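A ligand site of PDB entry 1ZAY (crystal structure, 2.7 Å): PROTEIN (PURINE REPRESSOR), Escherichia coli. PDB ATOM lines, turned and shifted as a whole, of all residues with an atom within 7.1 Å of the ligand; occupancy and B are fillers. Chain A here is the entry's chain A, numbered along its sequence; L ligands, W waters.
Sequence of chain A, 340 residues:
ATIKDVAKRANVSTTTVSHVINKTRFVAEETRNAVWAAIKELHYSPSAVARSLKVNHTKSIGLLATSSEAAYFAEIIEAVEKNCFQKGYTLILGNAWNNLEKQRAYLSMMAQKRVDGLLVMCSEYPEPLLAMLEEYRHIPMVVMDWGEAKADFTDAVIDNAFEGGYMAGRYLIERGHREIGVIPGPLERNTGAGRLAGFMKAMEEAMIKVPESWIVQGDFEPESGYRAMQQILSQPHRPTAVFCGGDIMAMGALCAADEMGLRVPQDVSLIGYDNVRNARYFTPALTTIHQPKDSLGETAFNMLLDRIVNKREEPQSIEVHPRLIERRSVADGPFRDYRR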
ATOM      1  N   THR A  66      31.503 -14.482  -3.078  1.00  0.00           N
ATOM      2  CA  THR A  66      31.780 -15.469  -2.082  1.00  0.00           C
ATOM      3  C   THR A  66      33.129 -16.109  -2.366  1.00  0.00           C
ATOM      4  O   THR A  66      34.033 -16.057  -1.551  1.00  0.00           O
ATOM      5  CB  THR A  66      30.708 -16.519  -2.119  1.00  0.00           C
ATOM      6  OG1 THR A  66      29.455 -15.911  -1.789  1.00  0.00           O
ATOM      7  CG2 THR A  66      31.009 -17.646  -1.159  1.00  0.00           C
ATOM      8  N   ALA A  70      35.055 -21.676  -7.963  1.00  0.00           N
ATOM      9  CA  ALA A  70      33.926 -22.536  -8.315  1.00  0.00           C
ATOM     10  C   ALA A  70      33.356 -22.220  -9.677  1.00  0.00           C
ATOM     11  O   ALA A  70      33.013 -21.089  -9.983  1.00  0.00           O
ATOM     12  CB  ALA A  70      32.858 -22.435  -7.286  1.00  0.00           C
ATOM     13  N   ALA A  71      33.257 -23.255 -10.482  1.00  0.00           N
ATOM     14  CA  ALA A  71      32.747 -23.136 -11.825  1.00  0.00           C
ATOM     15  C   ALA A  71      31.559 -22.241 -11.913  1.00  0.00           C
ATOM     16  O   ALA A  71      31.544 -21.303 -12.673  1.00  0.00           O
ATOM     17  CB  ALA A  71      32.396 -24.506 -12.361  1.00  0.00           C
ATOM     18  N   TYR A  72      30.544 -22.554 -11.119  1.00  0.00           N
ATOM     19  CA  TYR A  72      29.315 -21.779 -11.090  1.00  0.00           C
ATOM     20  C   TYR A  72      29.651 -20.312 -10.995  1.00  0.00           C
ATOM     21  O   TYR A  72      29.254 -19.513 -11.837  1.00  0.00           O
ATOM     22  CB  TYR A  72      28.488 -22.205  -9.888  1.00  0.00           C
ATOM     23  CG  TYR A  72      27.172 -21.491  -9.743  1.00  0.00           C
ATOM     24  CD1 TYR A  72      26.242 -21.471 -10.758  1.00  0.00           C
ATOM     25  CD2 TYR A  72      26.851 -20.831  -8.566  1.00  0.00           C
ATOM     26  CE1 TYR A  72      25.031 -20.803 -10.609  1.00  0.00           C
ATOM     27  CE2 TYR A  72      25.657 -20.167  -8.407  1.00  0.00           C
ATOM     28  CZ  TYR A  72      24.753 -20.159  -9.431  1.00  0.00           C
ATOM     29  OH  TYR A  72      23.573 -19.496  -9.275  1.00  0.00           O
ATOM     30  N   PHE A  73      30.410 -19.960  -9.980  1.00  0.00           N
ATOM     31  CA  PHE A  73      30.781 -18.588  -9.788  1.00  0.00           C
ATOM     32  C   PHE A  73      31.544 -18.003 -10.919  1.00  0.00           C
ATOM     33  O   PHE A  73      31.104 -17.034 -11.544  1.00  0.00           O
ATOM     34  CB  PHE A  73      31.562 -18.455  -8.507  1.00  0.00           C
ATOM     35  CG  PHE A  73      30.725 -18.675  -7.301  1.00  0.00           C
ATOM     36  CD1 PHE A  73      29.388 -18.339  -7.316  1.00  0.00           C
ATOM     37  CD2 PHE A  73      31.250 -19.230  -6.161  1.00  0.00           C
ATOM     38  CE1 PHE A  73      28.617 -18.555  -6.235  1.00  0.00           C
ATOM     39  CE2 PHE A  73      30.465 -19.445  -5.077  1.00  0.00           C
ATOM     40  CZ  PHE A  73      29.158 -19.107  -5.120  1.00  0.00           C
ATOM     41  N   SER A 123      25.891 -15.713  -1.020  1.00  0.00           N
ATOM     42  CA  SER A 123      25.424 -17.057  -0.697  1.00  0.00           C
ATOM     43  C   SER A 123      24.579 -17.107   0.533  1.00  0.00           C
ATOM     44  O   SER A 123      23.390 -17.317   0.425  1.00  0.00           O
ATOM     45  CB  SER A 123      26.613 -18.004  -0.554  1.00  0.00           C
ATOM     46  OG  SER A 123      27.463 -17.923  -1.682  1.00  0.00           O
ATOM     47  N   ASP A 159      16.419 -16.339  -9.545  1.00  0.00           N
ATOM     48  CA  ASP A 159      16.625 -17.577 -10.306  1.00  0.00           C
ATOM     49  C   ASP A 159      15.538 -18.629 -10.376  1.00  0.00           C
ATOM     50  O   ASP A 159      15.589 -19.502 -11.222  1.00  0.00           O
ATOM     51  CB  ASP A 159      17.930 -18.239  -9.904  1.00  0.00           C
ATOM     52  CG  ASP A 159      17.962 -18.580  -8.462  1.00  0.00           C
ATOM     53  OD1 ASP A 159      16.854 -18.759  -7.929  1.00  0.00           O
ATOM     54  OD2 ASP A 159      19.069 -18.628  -7.860  1.00  0.00           O
ATOM     55  N   PRO A 186      24.041 -26.498   0.784  1.00  0.00           N
ATOM     56  CA  PRO A 186      23.688 -25.827   2.036  1.00  0.00           C
ATOM     57  C   PRO A 186      22.290 -25.266   2.017  1.00  0.00           C
ATOM     58  O   PRO A 186      21.825 -24.714   1.010  1.00  0.00           O
ATOM     59  CB  PRO A 186      24.718 -24.706   2.111  1.00  0.00           C
ATOM     60  CG  PRO A 186      25.913 -25.300   1.530  1.00  0.00           C
ATOM     61  CD  PRO A 186      25.427 -26.177   0.385  1.00  0.00           C
ATOM     62  N   ARG A 189      21.428 -21.565   1.847  1.00  0.00           N
ATOM     63  CA  ARG A 189      21.534 -21.043   0.488  1.00  0.00           C
ATOM     64  C   ARG A 189      20.235 -21.247  -0.275  1.00  0.00           C
ATOM     65  O   ARG A 189      19.508 -22.193  -0.030  1.00  0.00           O
ATOM     66  CB  ARG A 189      22.640 -21.766  -0.272  1.00  0.00           C
ATOM     67  CG  ARG A 189      23.870 -20.954  -0.492  1.00  0.00           C
ATOM     68  CD  ARG A 189      24.992 -21.476   0.379  1.00  0.00           C
ATOM     69  NE  ARG A 189      26.257 -21.477  -0.345  1.00  0.00           N
ATOM     70  CZ  ARG A 189      27.434 -21.651   0.228  1.00  0.00           C
ATOM     71  NH1 ARG A 189      27.502 -21.829   1.543  1.00  0.00           N
ATOM     72  NH2 ARG A 189      28.548 -21.664  -0.489  1.00  0.00           N
ATOM     73  N   ASN A 190      19.971 -20.345  -1.211  1.00  0.00           N
ATOM     74  CA  ASN A 190      18.780 -20.409  -2.033  1.00  0.00           C
ATOM     75  C   ASN A 190      18.964 -21.561  -3.014  1.00  0.00           C
ATOM     76  O   ASN A 190      18.063 -22.387  -3.216  1.00  0.00           O
ATOM     77  CB  ASN A 190      18.637 -19.093  -2.801  1.00  0.00           C
ATOM     78  CG  ASN A 190      17.620 -19.179  -3.895  1.00  0.00           C
ATOM     79  OD1 ASN A 190      16.446 -19.440  -3.640  1.00  0.00           O
ATOM     80  ND2 ASN A 190      18.056 -18.961  -5.132  1.00  0.00           N
ATOM     81  N   THR A 191      20.140 -21.605  -3.610  1.00  0.00           N
ATOM     82  CA  THR A 191      20.517 -22.634  -4.562  1.00  0.00           C
ATOM     83  C   THR A 191      20.553 -24.021  -3.883  1.00  0.00           C
ATOM     84  O   THR A 191      20.636 -25.041  -4.569  1.00  0.00           O
ATOM     85  CB  THR A 191      21.896 -22.317  -5.204  1.00  0.00           C
ATOM     86  OG1 THR A 191      22.831 -21.969  -4.183  1.00  0.00           O
ATOM     87  CG2 THR A 191      21.786 -21.163  -6.170  1.00  0.00           C
ATOM     88  N   GLY A 192      20.499 -24.063  -2.548  1.00  0.00           N
ATOM     89  CA  GLY A 192      20.511 -25.327  -1.800  1.00  0.00           C
ATOM     90  C   GLY A 192      19.074 -25.614  -1.383  1.00  0.00           C
ATOM     91  O   GLY A 192      18.336 -26.344  -2.042  1.00  0.00           O
ATOM     92  N   ARG A 195      16.180 -25.395  -4.158  1.00  0.00           N
ATOM     93  CA  ARG A 195      16.101 -26.359  -5.241  1.00  0.00           C
ATOM     94  C   ARG A 195      15.522 -27.621  -4.623  1.00  0.00           C
ATOM     95  O   ARG A 195      14.677 -28.290  -5.202  1.00  0.00           O
ATOM     96  CB  ARG A 195      17.507 -26.604  -5.805  1.00  0.00           C
ATOM     97  CG  ARG A 195      18.137 -25.347  -6.486  1.00  0.00           C
ATOM     98  CD  ARG A 195      19.557 -25.616  -7.044  1.00  0.00           C
ATOM     99  NE  ARG A 195      20.074 -24.570  -7.939  1.00  0.00           N
ATOM    100  CZ  ARG A 195      21.349 -24.469  -8.289  1.00  0.00           C
ATOM    101  NH1 ARG A 195      22.249 -25.335  -7.823  1.00  0.00           N
ATOM    102  NH2 ARG A 195      21.754 -23.494  -9.109  1.00  0.00           N
ATOM    103  N   ASP A 219      28.343 -29.423   0.063  1.00  0.00           N
ATOM    104  CA  ASP A 219      28.760 -28.040   0.166  1.00  0.00           C
ATOM    105  C   ASP A 219      29.026 -27.463  -1.215  1.00  0.00           C
ATOM    106  O   ASP A 219      29.649 -26.422  -1.350  1.00  0.00           O
ATOM    107  CB  ASP A 219      30.024 -27.960   1.013  1.00  0.00           C
ATOM    108  CG  ASP A 219      31.073 -28.931   0.573  1.00  0.00           C
ATOM    109  OD1 ASP A 219      30.984 -29.407  -0.585  1.00  0.00           O
ATOM    110  OD2 ASP A 219      31.983 -29.223   1.356  1.00  0.00           O
ATOM    111  N   PHE A 220      28.560 -28.169  -2.246  1.00  0.00           N
ATOM    112  CA  PHE A 220      28.749 -27.753  -3.645  1.00  0.00           C
ATOM    113  C   PHE A 220      30.115 -28.106  -4.210  1.00  0.00           C
ATOM    114  O   PHE A 220      30.353 -27.903  -5.386  1.00  0.00           O
ATOM    115  CB  PHE A 220      28.498 -26.275  -3.844  1.00  0.00           C
ATOM    116  CG  PHE A 220      27.079 -25.933  -3.995  1.00  0.00           C
ATOM    117  CD1 PHE A 220      26.339 -26.460  -5.016  1.00  0.00           C
ATOM    118  CD2 PHE A 220      26.466 -25.063  -3.117  1.00  0.00           C
ATOM    119  CE1 PHE A 220      25.006 -26.141  -5.162  1.00  0.00           C
ATOM    120  CE2 PHE A 220      25.150 -24.748  -3.252  1.00  0.00           C
ATOM    121  CZ  PHE A 220      24.414 -25.284  -4.283  1.00  0.00           C
ATOM    122  N   GLU A 221      31.006 -28.650  -3.383  1.00  0.00           N
ATOM    123  CA  GLU A 221      32.352 -29.049  -3.798  1.00  0.00           C
ATOM    124  C   GLU A 221      32.380 -30.561  -4.129  1.00  0.00           C
ATOM    125  O   GLU A 221      31.803 -31.374  -3.391  1.00  0.00           O
ATOM    126  CB  GLU A 221      33.390 -28.708  -2.711  1.00  0.00           C
ATOM    127  CG  GLU A 221      33.609 -27.195  -2.508  1.00  0.00           C
ATOM    128  CD  GLU A 221      34.766 -26.619  -3.326  1.00  0.00           C
ATOM    129  OE1 GLU A 221      35.913 -26.611  -2.825  1.00  0.00           O
ATOM    130  OE2 GLU A 221      34.520 -26.171  -4.477  1.00  0.00           O
ATOM    131  N   GLY A 245      22.308 -31.492  -6.110  1.00  0.00           N
ATOM    132  CA  GLY A 245      22.193 -30.028  -6.007  1.00  0.00           C
ATOM    133  C   GLY A 245      22.959 -29.191  -7.003  1.00  0.00           C
ATOM    134  O   GLY A 245      22.467 -28.159  -7.439  1.00  0.00           O
ATOM    135  N   GLY A 246      24.171 -29.613  -7.364  1.00  0.00           N
ATOM    136  CA  GLY A 246      25.023 -28.877  -8.326  1.00  0.00           C
ATOM    137  C   GLY A 246      25.904 -29.795  -9.192  1.00  0.00           C
ATOM    138  O   GLY A 246      26.285 -30.897  -8.798  1.00  0.00           O
ATOM    139  N   ASP A 247      26.249 -29.337 -10.379  1.00  0.00           N
ATOM    140  CA  ASP A 247      27.069 -30.130 -11.270  1.00  0.00           C
ATOM    141  C   ASP A 247      28.451 -30.531 -10.732  1.00  0.00           C
ATOM    142  O   ASP A 247      28.838 -31.709 -10.749  1.00  0.00           O
ATOM    143  CB  ASP A 247      27.164 -29.472 -12.633  1.00  0.00           C
ATOM    144  CG  ASP A 247      25.803 -29.392 -13.336  1.00  0.00           C
ATOM    145  OD1 ASP A 247      24.794 -29.819 -12.753  1.00  0.00           O
ATOM    146  OD2 ASP A 247      25.771 -28.911 -14.488  1.00  0.00           O
ATOM    147  N   ILE A 248      29.202 -29.589 -10.221  1.00  0.00           N
ATOM    148  CA  ILE A 248      30.501 -29.976  -9.699  1.00  0.00           C
ATOM    149  C   ILE A 248      30.461 -31.000  -8.553  1.00  0.00           C
ATOM    150  O   ILE A 248      31.433 -31.700  -8.310  1.00  0.00           O
ATOM    151  CB  ILE A 248      31.354 -28.759  -9.356  1.00  0.00           C
ATOM    152  CG1 ILE A 248      31.667 -27.954 -10.623  1.00  0.00           C
ATOM    153  CG2 ILE A 248      32.610 -29.190  -8.627  1.00  0.00           C
ATOM    154  CD1 ILE A 248      32.858 -27.012 -10.474  1.00  0.00           C
ATOM    155  N   TYR A 273      22.449 -29.966 -11.354  1.00  0.00           N
ATOM    156  CA  TYR A 273      21.855 -28.665 -11.517  1.00  0.00           C
ATOM    157  C   TYR A 273      22.971 -27.676 -11.615  1.00  0.00           C
ATOM    158  O   TYR A 273      23.904 -27.723 -10.791  1.00  0.00           O
ATOM    159  CB  TYR A 273      21.028 -28.364 -10.252  1.00  0.00           C
ATOM    160  CG  TYR A 273      20.040 -27.245 -10.414  1.00  0.00           C
ATOM    161  CD1 TYR A 273      20.439 -26.002 -10.863  1.00  0.00           C
ATOM    162  CD2 TYR A 273      18.708 -27.421 -10.121  1.00  0.00           C
ATOM    163  CE1 TYR A 273      19.542 -24.960 -11.010  1.00  0.00           C
ATOM    164  CE2 TYR A 273      17.787 -26.363 -10.281  1.00  0.00           C
ATOM    165  CZ  TYR A 273      18.222 -25.146 -10.722  1.00  0.00           C
ATOM    166  OH  TYR A 273      17.344 -24.082 -10.891  1.00  0.00           O
ATOM    167  N   ASP A 274      22.855 -26.785 -12.600  1.00  0.00           N
ATOM    168  CA  ASP A 274      23.789 -25.679 -12.921  1.00  0.00           C
ATOM    169  C   ASP A 274      24.101 -25.551 -14.403  1.00  0.00           C
ATOM    170  O   ASP A 274      24.028 -24.473 -14.994  1.00  0.00           O
ATOM    171  CB  ASP A 274      25.124 -25.748 -12.152  1.00  0.00           C
ATOM    172  CG  ASP A 274      25.027 -25.129 -10.752  1.00  0.00           C
ATOM    173  OD1 ASP A 274      23.933 -24.642 -10.379  1.00  0.00           O
ATOM    174  OD2 ASP A 274      26.071 -25.139 -10.032  1.00  0.00           O
ATOM    175  N   VAL A 276      27.108 -26.352 -15.976  1.00  0.00           N
ATOM    176  CA  VAL A 276      28.391 -25.711 -16.097  1.00  0.00           C
ATOM    177  C   VAL A 276      28.962 -25.921 -17.495  1.00  0.00           C
ATOM    178  O   VAL A 276      28.593 -26.854 -18.212  1.00  0.00           O
ATOM    179  CB  VAL A 276      29.344 -26.284 -15.052  1.00  0.00           C
ATOM    180  CG1 VAL A 276      30.794 -26.052 -15.455  1.00  0.00           C
ATOM    181  CG2 VAL A 276      29.045 -25.680 -13.701  1.00  0.00           C
ATOM    182  N   GLN A 291      21.092 -23.247 -15.482  1.00  0.00           N
ATOM    183  CA  GLN A 291      20.916 -21.945 -14.862  1.00  0.00           C
ATOM    184  C   GLN A 291      21.527 -20.933 -15.808  1.00  0.00           C
ATOM    185  O   GLN A 291      22.710 -21.018 -16.141  1.00  0.00           O
ATOM    186  CB  GLN A 291      21.643 -21.842 -13.546  1.00  0.00           C
ATOM    187  CG  GLN A 291      21.524 -20.436 -12.975  1.00  0.00           C
ATOM    188  CD  GLN A 291      20.551 -20.352 -11.814  1.00  0.00           C
ATOM    189  OE1 GLN A 291      20.968 -20.098 -10.694  1.00  0.00           O
ATOM    190  NE2 GLN A 291      19.252 -20.547 -12.087  1.00  0.00           N
HETATM  191  N1  LIG L   1      28.333 -22.752  -5.076  1.00  0.00           N
HETATM  192  C1  LIG L   1      28.690 -23.492  -6.189  1.00  0.00           C
HETATM  193  N2  LIG L   1      27.841 -23.863  -7.145  1.00  0.00           N
HETATM  194  C2  LIG L   1      26.585 -23.436  -6.884  1.00  0.00           C
HETATM  195  C3  LIG L   1      26.128 -22.694  -5.823  1.00  0.00           C
HETATM  196  C4  LIG L   1      27.044 -22.292  -4.808  1.00  0.00           C
HETATM  197  O1  LIG L   1      26.818 -21.635  -3.786  1.00  0.00           O
HETATM  198  N3  LIG L   1      24.767 -22.450  -5.934  1.00  0.00           N
HETATM  199  C5  LIG L   1      24.431 -23.034  -7.048  1.00  0.00           C
HETATM  200  N4  LIG L   1      25.472 -23.658  -7.684  1.00  0.00           N
HETATM  201  O   HOH W   1      30.089 -24.868  -8.894  1.00  0.00           O
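OG1 of Thr 191 lies within hydrogen-bond range of N3 of the ligand (2.7 Å). The side-chain carboxylate (OD2) of Asp 274 lies within hydrogen-bond range of a nitrogen (N4) of the ligand (2.8 Å). O1 of the ligand is in hydrogen-bond range of NE of Arg 189, at 3.5 Å.
The guanidinium group (NE) of Arg 195 sits close to the backbone carbonyl oxygen (O) of Thr 191, at 3.4 Å. The side-chain carboxylate (OD1) of Asp 274 is in salt-bridge range of the guanidinium group (NH2) of Arg 195 (2.8 Å). The backbone NH (N) of Gln 291 lies within hydrogen-bond range of the backbone carbonyl oxygen (O) of Asp 274, at 3.2 Å. The side-chain amide oxygen (OE1) of Gln 291 lies within hydrogen-bond range of the side-chain hydroxyl (OH) of Tyr 72. The guanidinium group (NH1) of Arg 195 is in hydrogen-bond range of the backbone carbonyl oxygen (O) of Gly 245, 2.9 Å away.
Tyr 72 touches the ligand (CD2 to C2, 3.1 Å). CZ of Phe 73 touches O1 of the ligand, at 3.7 Å. Arg 195 touches the ligand. Phe 220 touches the ligand (CD2 to C4, 3.3 Å). Hydrophobic or aromatic side chains within 4 Å of the ligand: Tyr 72, Phe 73 and Phe 220. Within 4 Å of the ligand: Tyr 72, Phe 73, Arg 189, Thr 191, Arg 195, Phe 220 and Asp 274.
Water W1 lies within hydrogen-bond range of N2 of the ligand and N of Tyr 72.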
